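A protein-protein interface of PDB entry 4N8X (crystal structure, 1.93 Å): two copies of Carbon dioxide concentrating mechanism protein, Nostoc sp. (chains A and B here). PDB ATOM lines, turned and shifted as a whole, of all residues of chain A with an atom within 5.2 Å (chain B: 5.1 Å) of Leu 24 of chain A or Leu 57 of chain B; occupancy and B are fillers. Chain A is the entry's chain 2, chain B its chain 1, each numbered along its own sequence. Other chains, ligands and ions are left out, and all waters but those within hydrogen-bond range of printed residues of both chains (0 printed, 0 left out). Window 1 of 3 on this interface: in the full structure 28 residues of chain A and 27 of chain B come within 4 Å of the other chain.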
ATOM      1  N   GLY A   8      -0.265 -10.422  16.140  1.00  0.00           N
ATOM      2  CA  GLY A   8      -1.332  -9.690  15.497  1.00  0.00           C
ATOM      3  C   GLY A   8      -2.456 -10.514  14.903  1.00  0.00           C
ATOM      4  O   GLY A   8      -2.427 -11.759  14.904  1.00  0.00           O
ATOM      5  N   THR A   9      -3.463  -9.797  14.406  1.00  0.00           N
ATOM      6  CA  THR A   9      -4.552 -10.394  13.646  1.00  0.00           C
ATOM      7  C   THR A   9      -4.452  -9.963  12.176  1.00  0.00           C
ATOM      8  O   THR A   9      -4.044  -8.829  11.879  1.00  0.00           O
ATOM      9  CB  THR A   9      -5.895  -9.984  14.234  1.00  0.00           C
ATOM     10  OG1 THR A   9      -5.835 -10.138  15.656  1.00  0.00           O
ATOM     11  CG2 THR A   9      -7.030 -10.863  13.676  1.00  0.00           C
ATOM     12  N   VAL A  10      -4.768 -10.882  11.267  1.00  0.00           N
ATOM     13  CA  VAL A  10      -4.854 -10.592   9.840  1.00  0.00           C
ATOM     14  C   VAL A  10      -6.306 -10.765   9.454  1.00  0.00           C
ATOM     15  O   VAL A  10      -6.882 -11.803   9.754  1.00  0.00           O
ATOM     16  CB  VAL A  10      -4.010 -11.533   9.020  1.00  0.00           C
ATOM     17  CG1 VAL A  10      -4.156 -11.189   7.509  1.00  0.00           C
ATOM     18  CG2 VAL A  10      -2.546 -11.417   9.436  1.00  0.00           C
ATOM     19  N   SER A  12      -9.186 -10.723   6.354  1.00  0.00           N
ATOM     20  CA  SER A  12      -9.386 -10.770   4.915  1.00  0.00           C
ATOM     21  C   SER A  12     -10.872 -10.880   4.657  1.00  0.00           C
ATOM     22  O   SER A  12     -11.549 -11.620   5.361  1.00  0.00           O
ATOM     23  CB  SER A  12      -8.671 -11.984   4.344  1.00  0.00           C
ATOM     24  OG  SER A  12      -9.098 -12.269   3.013  1.00  0.00           O
ATOM     25  N   LYS A  15     -11.155 -14.070  -0.245  1.00  0.00           N
ATOM     26  CA  LYS A  15     -10.277 -15.197   0.054  1.00  0.00           C
ATOM     27  C   LYS A  15     -10.831 -16.424  -0.575  1.00  0.00           C
ATOM     28  O   LYS A  15     -12.002 -16.430  -1.004  1.00  0.00           O
ATOM     29  CB  LYS A  15     -10.195 -15.423   1.586  1.00  0.00           C
ATOM     30  CG  LYS A  15     -11.571 -15.798   2.187  1.00  0.00           C
ATOM     31  CD  LYS A  15     -11.561 -15.898   3.717  1.00  0.00           C
ATOM     32  CE  LYS A  15     -11.125 -14.592   4.376  1.00  0.00           C
ATOM     33  NZ  LYS A  15     -11.505 -14.523   5.848  1.00  0.00           N
ATOM     34  N   LEU A  19     -11.186 -20.849   3.197  1.00  0.00           N
ATOM     35  CA  LEU A  19     -10.637 -20.083   4.304  1.00  0.00           C
ATOM     36  C   LEU A  19     -11.698 -19.254   5.040  1.00  0.00           C
ATOM     37  O   LEU A  19     -11.394 -18.578   6.023  1.00  0.00           O
ATOM     38  CB  LEU A  19      -9.476 -19.219   3.843  1.00  0.00           C
ATOM     39  CG  LEU A  19      -8.127 -19.868   3.553  1.00  0.00           C
ATOM     40  CD1 LEU A  19      -7.066 -18.773   3.612  1.00  0.00           C
ATOM     41  CD2 LEU A  19      -7.774 -21.020   4.504  1.00  0.00           C
ATOM     42  N   VAL A  22     -11.933 -18.995   9.061  1.00  0.00           N
ATOM     43  CA  VAL A  22     -10.655 -19.380   9.664  1.00  0.00           C
ATOM     44  C   VAL A  22      -9.937 -18.186  10.279  1.00  0.00           C
ATOM     45  O   VAL A  22      -9.609 -17.240   9.591  1.00  0.00           O
ATOM     46  CB  VAL A  22      -9.712 -19.991   8.628  1.00  0.00           C
ATOM     47  CG1 VAL A  22      -8.280 -20.111   9.210  1.00  0.00           C
ATOM     48  CG2 VAL A  22     -10.235 -21.336   8.160  1.00  0.00           C
ATOM     49  N   LYS A  23      -9.662 -18.229  11.572  1.00  0.00           N
ATOM     50  CA  LYS A  23      -8.966 -17.118  12.232  1.00  0.00           C
ATOM     51  C   LYS A  23      -7.499 -17.096  11.789  1.00  0.00           C
ATOM     52  O   LYS A  23      -6.808 -18.119  11.846  1.00  0.00           O
ATOM     53  CB  LYS A  23      -9.091 -17.278  13.755  1.00  0.00           C
ATOM     54  CG  LYS A  23      -8.503 -16.156  14.616  1.00  0.00           C
ATOM     55  CD  LYS A  23      -8.850 -16.362  16.097  1.00  0.00           C
ATOM     56  CE  LYS A  23      -8.246 -15.260  16.984  1.00  0.00           C
ATOM     57  NZ  LYS A  23      -7.461 -15.820  18.138  1.00  0.00           N
ATOM     58  N   LEU A  24      -7.030 -15.945  11.309  1.00  0.00           N
ATOM     59  CA  LEU A  24      -5.678 -15.807  10.780  1.00  0.00           C
ATOM     60  C   LEU A  24      -4.847 -14.937  11.725  1.00  0.00           C
ATOM     61  O   LEU A  24      -5.110 -13.736  11.843  1.00  0.00           O
ATOM     62  CB  LEU A  24      -5.707 -15.164   9.379  1.00  0.00           C
ATOM     63  CG  LEU A  24      -6.474 -15.887   8.255  1.00  0.00           C
ATOM     64  CD1 LEU A  24      -6.588 -15.039   6.974  1.00  0.00           C
ATOM     65  CD2 LEU A  24      -5.837 -17.242   7.937  1.00  0.00           C
ATOM     66  N   LEU A  25      -3.835 -15.530  12.372  1.00  0.00           N
ATOM     67  CA  LEU A  25      -2.993 -14.811  13.326  1.00  0.00           C
ATOM     68  C   LEU A  25      -1.597 -14.581  12.803  1.00  0.00           C
ATOM     69  O   LEU A  25      -1.024 -15.456  12.191  1.00  0.00           O
ATOM     70  CB  LEU A  25      -2.873 -15.586  14.636  1.00  0.00           C
ATOM     71  CG  LEU A  25      -4.102 -15.847  15.501  1.00  0.00           C
ATOM     72  CD1 LEU A  25      -3.680 -16.617  16.750  1.00  0.00           C
ATOM     73  CD2 LEU A  25      -4.801 -14.509  15.886  1.00  0.00           C
ATOM     74  N   LEU A  26      -1.043 -13.400  13.068  1.00  0.00           N
ATOM     75  CA  LEU A  26       0.365 -13.112  12.797  1.00  0.00           C
ATOM     76  C   LEU A  26       1.233 -13.581  13.977  1.00  0.00           C
ATOM     77  O   LEU A  26       1.131 -13.069  15.115  1.00  0.00           O
ATOM     78  CB  LEU A  26       0.594 -11.613  12.582  1.00  0.00           C
ATOM     79  CG  LEU A  26       2.034 -11.171  12.300  1.00  0.00           C
ATOM     80  CD1 LEU A  26       2.510 -11.711  10.950  1.00  0.00           C
ATOM     81  CD2 LEU A  26       2.116  -9.654  12.319  1.00  0.00           C
ATOM     82  N   VAL A  42       1.842 -16.339   9.073  1.00  0.00           N
ATOM     83  CA  VAL A  42       0.436 -16.105   9.317  1.00  0.00           C
ATOM     84  C   VAL A  42      -0.136 -17.491   9.411  1.00  0.00           C
ATOM     85  O   VAL A  42       0.002 -18.301   8.488  1.00  0.00           O
ATOM     86  CB  VAL A  42      -0.244 -15.271   8.203  1.00  0.00           C
ATOM     87  CG1 VAL A  42      -1.779 -15.272   8.415  1.00  0.00           C
ATOM     88  CG2 VAL A  42       0.336 -13.831   8.238  1.00  0.00           C
ATOM     89  N   ALA A  43      -0.753 -17.781  10.549  1.00  0.00           N
ATOM     90  CA  ALA A  43      -1.178 -19.123  10.811  1.00  0.00           C
ATOM     91  C   ALA A  43      -2.657 -19.185  11.077  1.00  0.00           C
ATOM     92  O   ALA A  43      -3.242 -18.224  11.592  1.00  0.00           O
ATOM     93  CB  ALA A  43      -0.422 -19.683  12.013  1.00  0.00           C
ATOM     94  N   ALA A  44      -3.253 -20.334  10.740  1.00  0.00           N
ATOM     95  CA  ALA A  44      -4.670 -20.597  11.040  1.00  0.00           C
ATOM     96  C   ALA A  44      -4.760 -20.919  12.518  1.00  0.00           C
ATOM     97  O   ALA A  44      -3.867 -21.590  13.063  1.00  0.00           O
ATOM     98  CB  ALA A  44      -5.155 -21.762  10.251  1.00  0.00           C
ATOM     99  N   ASP A  45      -5.833 -20.468  13.170  1.00  0.00           N
ATOM    100  CA  ASP A  45      -6.025 -20.758  14.585  1.00  0.00           C
ATOM    101  C   ASP A  45      -7.488 -21.042  14.881  1.00  0.00           C
ATOM    102  O   ASP A  45      -8.134 -20.289  15.595  1.00  0.00           O
ATOM    103  CB  ASP A  45      -5.541 -19.589  15.447  1.00  0.00           C
ATOM    104  CG  ASP A  45      -5.711 -19.853  16.937  1.00  0.00           C
ATOM    105  OD1 ASP A  45      -5.708 -21.038  17.336  1.00  0.00           O
ATOM    106  OD2 ASP A  45      -5.873 -18.880  17.710  1.00  0.00           O
ATOM    107  N   MET B   1       1.575 -19.153   6.376  1.00  0.00           N
ATOM    108  CA  MET B   1       1.504 -18.372   5.162  1.00  0.00           C
ATOM    109  C   MET B   1       2.352 -17.118   5.277  1.00  0.00           C
ATOM    110  O   MET B   1       2.496 -16.572   6.352  1.00  0.00           O
ATOM    111  CB  MET B   1       0.055 -17.946   4.914  1.00  0.00           C
ATOM    112  CG  MET B   1      -0.889 -19.098   4.525  1.00  0.00           C
ATOM    113  SD  MET B   1      -1.268 -20.189   5.900  1.00  0.00           S
ATOM    114  CE  MET B   1      -2.554 -19.282   6.823  1.00  0.00           C
ATOM    115  N   GLN B   2       2.894 -16.657   4.157  1.00  0.00           N
ATOM    116  CA  GLN B   2       3.649 -15.418   4.123  1.00  0.00           C
ATOM    117  C   GLN B   2       2.792 -14.322   3.541  1.00  0.00           C
ATOM    118  O   GLN B   2       1.880 -14.581   2.758  1.00  0.00           O
ATOM    119  CB  GLN B   2       4.951 -15.586   3.289  1.00  0.00           C
ATOM    120  CG  GLN B   2       6.049 -16.478   3.964  1.00  0.00           C
ATOM    121  CD  GLN B   2       6.436 -16.039   5.401  1.00  0.00           C
ATOM    122  OE1 GLN B   2       7.301 -15.163   5.602  1.00  0.00           O
ATOM    123  NE2 GLN B   2       5.824 -16.676   6.402  1.00  0.00           N
ATOM    124  N   ILE B   3       3.133 -13.083   3.886  1.00  0.00           N
ATOM    125  CA  ILE B   3       2.484 -11.880   3.367  1.00  0.00           C
ATOM    126  C   ILE B   3       3.321 -11.388   2.194  1.00  0.00           C
ATOM    127  O   ILE B   3       4.544 -11.378   2.274  1.00  0.00           O
ATOM    128  CB  ILE B   3       2.473 -10.786   4.488  1.00  0.00           C
ATOM    129  CG1 ILE B   3       1.640 -11.268   5.663  1.00  0.00           C
ATOM    130  CG2 ILE B   3       1.907  -9.409   4.008  1.00  0.00           C
ATOM    131  CD1 ILE B   3       1.957 -10.546   6.932  1.00  0.00           C
ATOM    132  N   TRP B  55      -1.854  -6.444  -0.913  1.00  0.00           N
ATOM    133  CA  TRP B  55      -1.241  -7.428  -0.037  1.00  0.00           C
ATOM    134  C   TRP B  55      -2.084  -8.708   0.025  1.00  0.00           C
ATOM    135  O   TRP B  55      -3.312  -8.680   0.157  1.00  0.00           O
ATOM    136  CB  TRP B  55      -1.084  -6.836   1.371  1.00  0.00           C
ATOM    137  CG  TRP B  55       0.021  -5.795   1.472  1.00  0.00           C
ATOM    138  CD1 TRP B  55       0.476  -4.977   0.476  1.00  0.00           C
ATOM    139  CD2 TRP B  55       0.802  -5.482   2.639  1.00  0.00           C
ATOM    140  NE1 TRP B  55       1.499  -4.157   0.956  1.00  0.00           N
ATOM    141  CE2 TRP B  55       1.713  -4.452   2.273  1.00  0.00           C
ATOM    142  CE3 TRP B  55       0.806  -5.956   3.954  1.00  0.00           C
ATOM    143  CZ2 TRP B  55       2.627  -3.894   3.181  1.00  0.00           C
ATOM    144  CZ3 TRP B  55       1.738  -5.398   4.862  1.00  0.00           C
ATOM    145  CH2 TRP B  55       2.621  -4.377   4.460  1.00  0.00           C
ATOM    146  N   VAL B  56      -1.410  -9.842  -0.032  1.00  0.00           N
ATOM    147  CA  VAL B  56      -2.088 -11.114  -0.076  1.00  0.00           C
ATOM    148  C   VAL B  56      -1.334 -12.079   0.845  1.00  0.00           C
ATOM    149  O   VAL B  56      -0.197 -11.816   1.215  1.00  0.00           O
ATOM    150  CB  VAL B  56      -2.071 -11.673  -1.514  1.00  0.00           C
ATOM    151  CG1 VAL B  56      -2.887 -10.765  -2.440  1.00  0.00           C
ATOM    152  CG2 VAL B  56      -0.625 -11.773  -2.031  1.00  0.00           C
ATOM    153  N   LEU B  57      -1.997 -13.171   1.220  1.00  0.00           N
ATOM    154  CA  LEU B  57      -1.341 -14.286   1.865  1.00  0.00           C
ATOM    155  C   LEU B  57      -1.020 -15.350   0.814  1.00  0.00           C
ATOM    156  O   LEU B  57      -1.865 -15.683  -0.026  1.00  0.00           O
ATOM    157  CB  LEU B  57      -2.267 -14.882   2.912  1.00  0.00           C
ATOM    158  CG  LEU B  57      -2.551 -13.951   4.060  1.00  0.00           C
ATOM    159  CD1 LEU B  57      -3.679 -14.542   4.863  1.00  0.00           C
ATOM    160  CD2 LEU B  57      -1.278 -13.916   4.912  1.00  0.00           C
ATOM    161  N   ILE B  58       0.180 -15.901   0.913  1.00  0.00           N
ATOM    162  CA  ILE B  58       0.641 -16.989   0.059  1.00  0.00           C
ATOM    163  C   ILE B  58       0.766 -18.265   0.910  1.00  0.00           C
ATOM    164  O   ILE B  58       1.368 -18.237   1.974  1.00  0.00           O
ATOM    165  CB  ILE B  58       2.039 -16.681  -0.452  1.00  0.00           C
ATOM    166  CG1 ILE B  58       2.075 -15.384  -1.298  1.00  0.00           C
ATOM    167  CG2 ILE B  58       2.542 -17.836  -1.358  1.00  0.00           C
ATOM    168  CD1 ILE B  58       3.531 -15.109  -1.845  1.00  0.00           C
ATOM    169  N   SER B  59       0.186 -19.374   0.444  1.00  0.00           N
ATOM    170  CA  SER B  59       0.421 -20.685   1.034  1.00  0.00           C
ATOM    171  C   SER B  59       1.402 -21.410   0.148  1.00  0.00           C
ATOM    172  O   SER B  59       1.273 -21.358  -1.089  1.00  0.00           O
ATOM    173  CB  SER B  59      -0.902 -21.450   1.119  1.00  0.00           C
ATOM    174  OG  SER B  59      -1.606 -21.044   2.275  1.00  0.00           O
ATOM    175  N   ALA B  78       0.483 -20.447  -3.855  1.00  0.00           N
ATOM    176  CA  ALA B  78      -0.834 -19.984  -4.270  1.00  0.00           C
ATOM    177  C   ALA B  78      -1.273 -18.775  -3.429  1.00  0.00           C
ATOM    178  O   ALA B  78      -1.011 -18.710  -2.216  1.00  0.00           O
ATOM    179  CB  ALA B  78      -1.889 -21.159  -4.197  1.00  0.00           C
ATOM    180  N   VAL B  79      -1.964 -17.844  -4.077  1.00  0.00           N
ATOM    181  CA  VAL B  79      -2.630 -16.763  -3.376  1.00  0.00           C
ATOM    182  C   VAL B  79      -3.895 -17.299  -2.709  1.00  0.00           C
ATOM    183  O   VAL B  79      -4.700 -17.949  -3.346  1.00  0.00           O
ATOM    184  CB  VAL B  79      -2.916 -15.596  -4.336  1.00  0.00           C
ATOM    185  CG1 VAL B  79      -3.815 -14.548  -3.678  1.00  0.00           C
ATOM    186  CG2 VAL B  79      -1.594 -14.978  -4.800  1.00  0.00           C
ATOM    187  N   VAL B  80      -4.037 -17.114  -1.387  1.00  0.00           N
ATOM    188  CA  VAL B  80      -5.195 -17.688  -0.732  1.00  0.00           C
ATOM    189  C   VAL B  80      -6.120 -16.634  -0.154  1.00  0.00           C
ATOM    190  O   VAL B  80      -7.281 -16.913   0.154  1.00  0.00           O
ATOM    191  CB  VAL B  80      -4.824 -18.780   0.340  1.00  0.00           C
ATOM    192  CG1 VAL B  80      -4.004 -19.893  -0.287  1.00  0.00           C
ATOM    193  CG2 VAL B  80      -4.051 -18.188   1.555  1.00  0.00           C
ATOM    194  N   ALA B  81      -5.615 -15.419  -0.003  1.00  0.00           N
ATOM    195  CA  ALA B  81      -6.430 -14.370   0.605  1.00  0.00           C
ATOM    196  C   ALA B  81      -5.879 -13.002   0.231  1.00  0.00           C
ATOM    197  O   ALA B  81      -4.677 -12.861   0.032  1.00  0.00           O
ATOM    198  CB  ALA B  81      -6.437 -14.542   2.134  1.00  0.00           C
ATOM    199  N   ILE B  82      -6.762 -12.010   0.136  1.00  0.00           N
ATOM    200  CA  ILE B  82      -6.347 -10.612   0.036  1.00  0.00           C
ATOM    201  C   ILE B  82      -6.516  -9.977   1.426  1.00  0.00           C
ATOM    202  O   ILE B  82      -7.565 -10.098   2.072  1.00  0.00           O
ATOM    203  CB  ILE B  82      -7.213  -9.836  -0.983  1.00  0.00           C
ATOM    204  CG1 ILE B  82      -6.987 -10.382  -2.393  1.00  0.00           C
ATOM    205  CG2 ILE B  82      -6.963  -8.288  -0.900  1.00  0.00           C
ATOM    206  CD1 ILE B  82      -8.196 -10.135  -3.362  1.00  0.00           C
ATOM    207  N   ILE B  83      -5.477  -9.314   1.905  1.00  0.00           N
ATOM    208  CA  ILE B  83      -5.520  -8.729   3.243  1.00  0.00           C
ATOM    209  C   ILE B  83      -6.155  -7.358   3.197  1.00  0.00           C
ATOM    210  O   ILE B  83      -5.794  -6.545   2.328  1.00  0.00           O
ATOM    211  CB  ILE B  83      -4.096  -8.607   3.820  1.00  0.00           C
ATOM    212  CG1 ILE B  83      -3.443  -9.996   3.913  1.00  0.00           C
ATOM    213  CG2 ILE B  83      -4.164  -8.013   5.192  1.00  0.00           C
ATOM    214  CD1 ILE B  83      -1.950  -9.951   3.887  1.00  0.00           C
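The backbone NH (N) of Met 1 of chain B sits at hydrogen-bond distance from the backbone carbonyl oxygen (O) of Val 42 of chain A. The backbone carbonyl oxygen (O) of Ile 82 of chain B sits at hydrogen-bond distance from the side-chain hydroxyl (OG) of Ser 12 of chain A, 2.8 Å away.
OG of Ser 59 of chain B sits close to SD of Met 1 of chain B, 3.7 Å away. O of Trp 55 of chain B is in hydrogen-bond range of N of Ile 83 of chain B (2.9 Å). The backbone carbonyl oxygen of Leu 57 of chain B is in hydrogen-bond range of the backbone NH of Val 80 of chain B (2.9 Å). N of Leu 57 of chain B sits at hydrogen-bond distance from O of Ala 81 of chain B, at 2.9 Å. O of Leu 24 of chain A lies within hydrogen-bond range of N of Val 10 of chain A, at 2.9 Å. The side-chain amino group (NZ) of Lys 15 of chain A is in hydrogen-bond range of the backbone carbonyl oxygen (O) of Ser 12 of chain A (2.9 Å).
Of chain B, only Leu 57 comes within 4 Å of Leu 24 of chain A. Printed residues of chain A within 4 Å of Met 1 of chain B: Val 42. Printed residues of chain A within 4 Å of Leu 57 of chain B: Leu 24 (3.6 Å) and Val 42 (3.7 Å). Printed residues of chain A within 4 Å of Val 80 of chain B: Lys 15 and Leu 19. Printed residues of chain A within 4 Å of Ile 82 of chain B: Ser 12. The nearest residue of chain B that does not touch Leu 24 of chain A is Met 1 of chain B (4.02 Å). The nearest residue of chain A that does not touch Leu 57 of chain B is Val 10 of chain A (4.3 Å). The nearest printed residue of chain A that does not touch Ile 82 of chain B is Lys 15 of chain A (4.7 Å).
Of the 15 printed residues of chain A, 6 touch a printed residue of chain B. Hydrophobic or aromatic side chains of chain A within 4 Å of the printed part of chain B: Val 10, Leu 19, Leu 24 and Val 42. Among the printed residues, no Asp or Glu carboxylate lies within 4 Å of a Lys or Arg side-chain nitrogen of the other chain.
No position is printed for both chains.
Among the printed residues, pairs that only touch across the chains: Val 10 of chain A with Ile 83 of chain B (3.9 Å), Ser 12 of chain A with Ala 81 of chain B (3.6 Å), Lys 15 of chain A with Val 80 of chain B (3.5 Å), Lys 15 of chain A with Ala 81 of chain B (3.9 Å), Leu 19 of chain A with Val 80 of chain B (3.7 Å), Leu 24 of chain A with Leu 57 of chain B (3.6 Å), Val 42 of chain A with Ile 3 of chain B (3.9 Å) and Val 42 of chain A with Leu 57 of chain B (3.7 Å).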
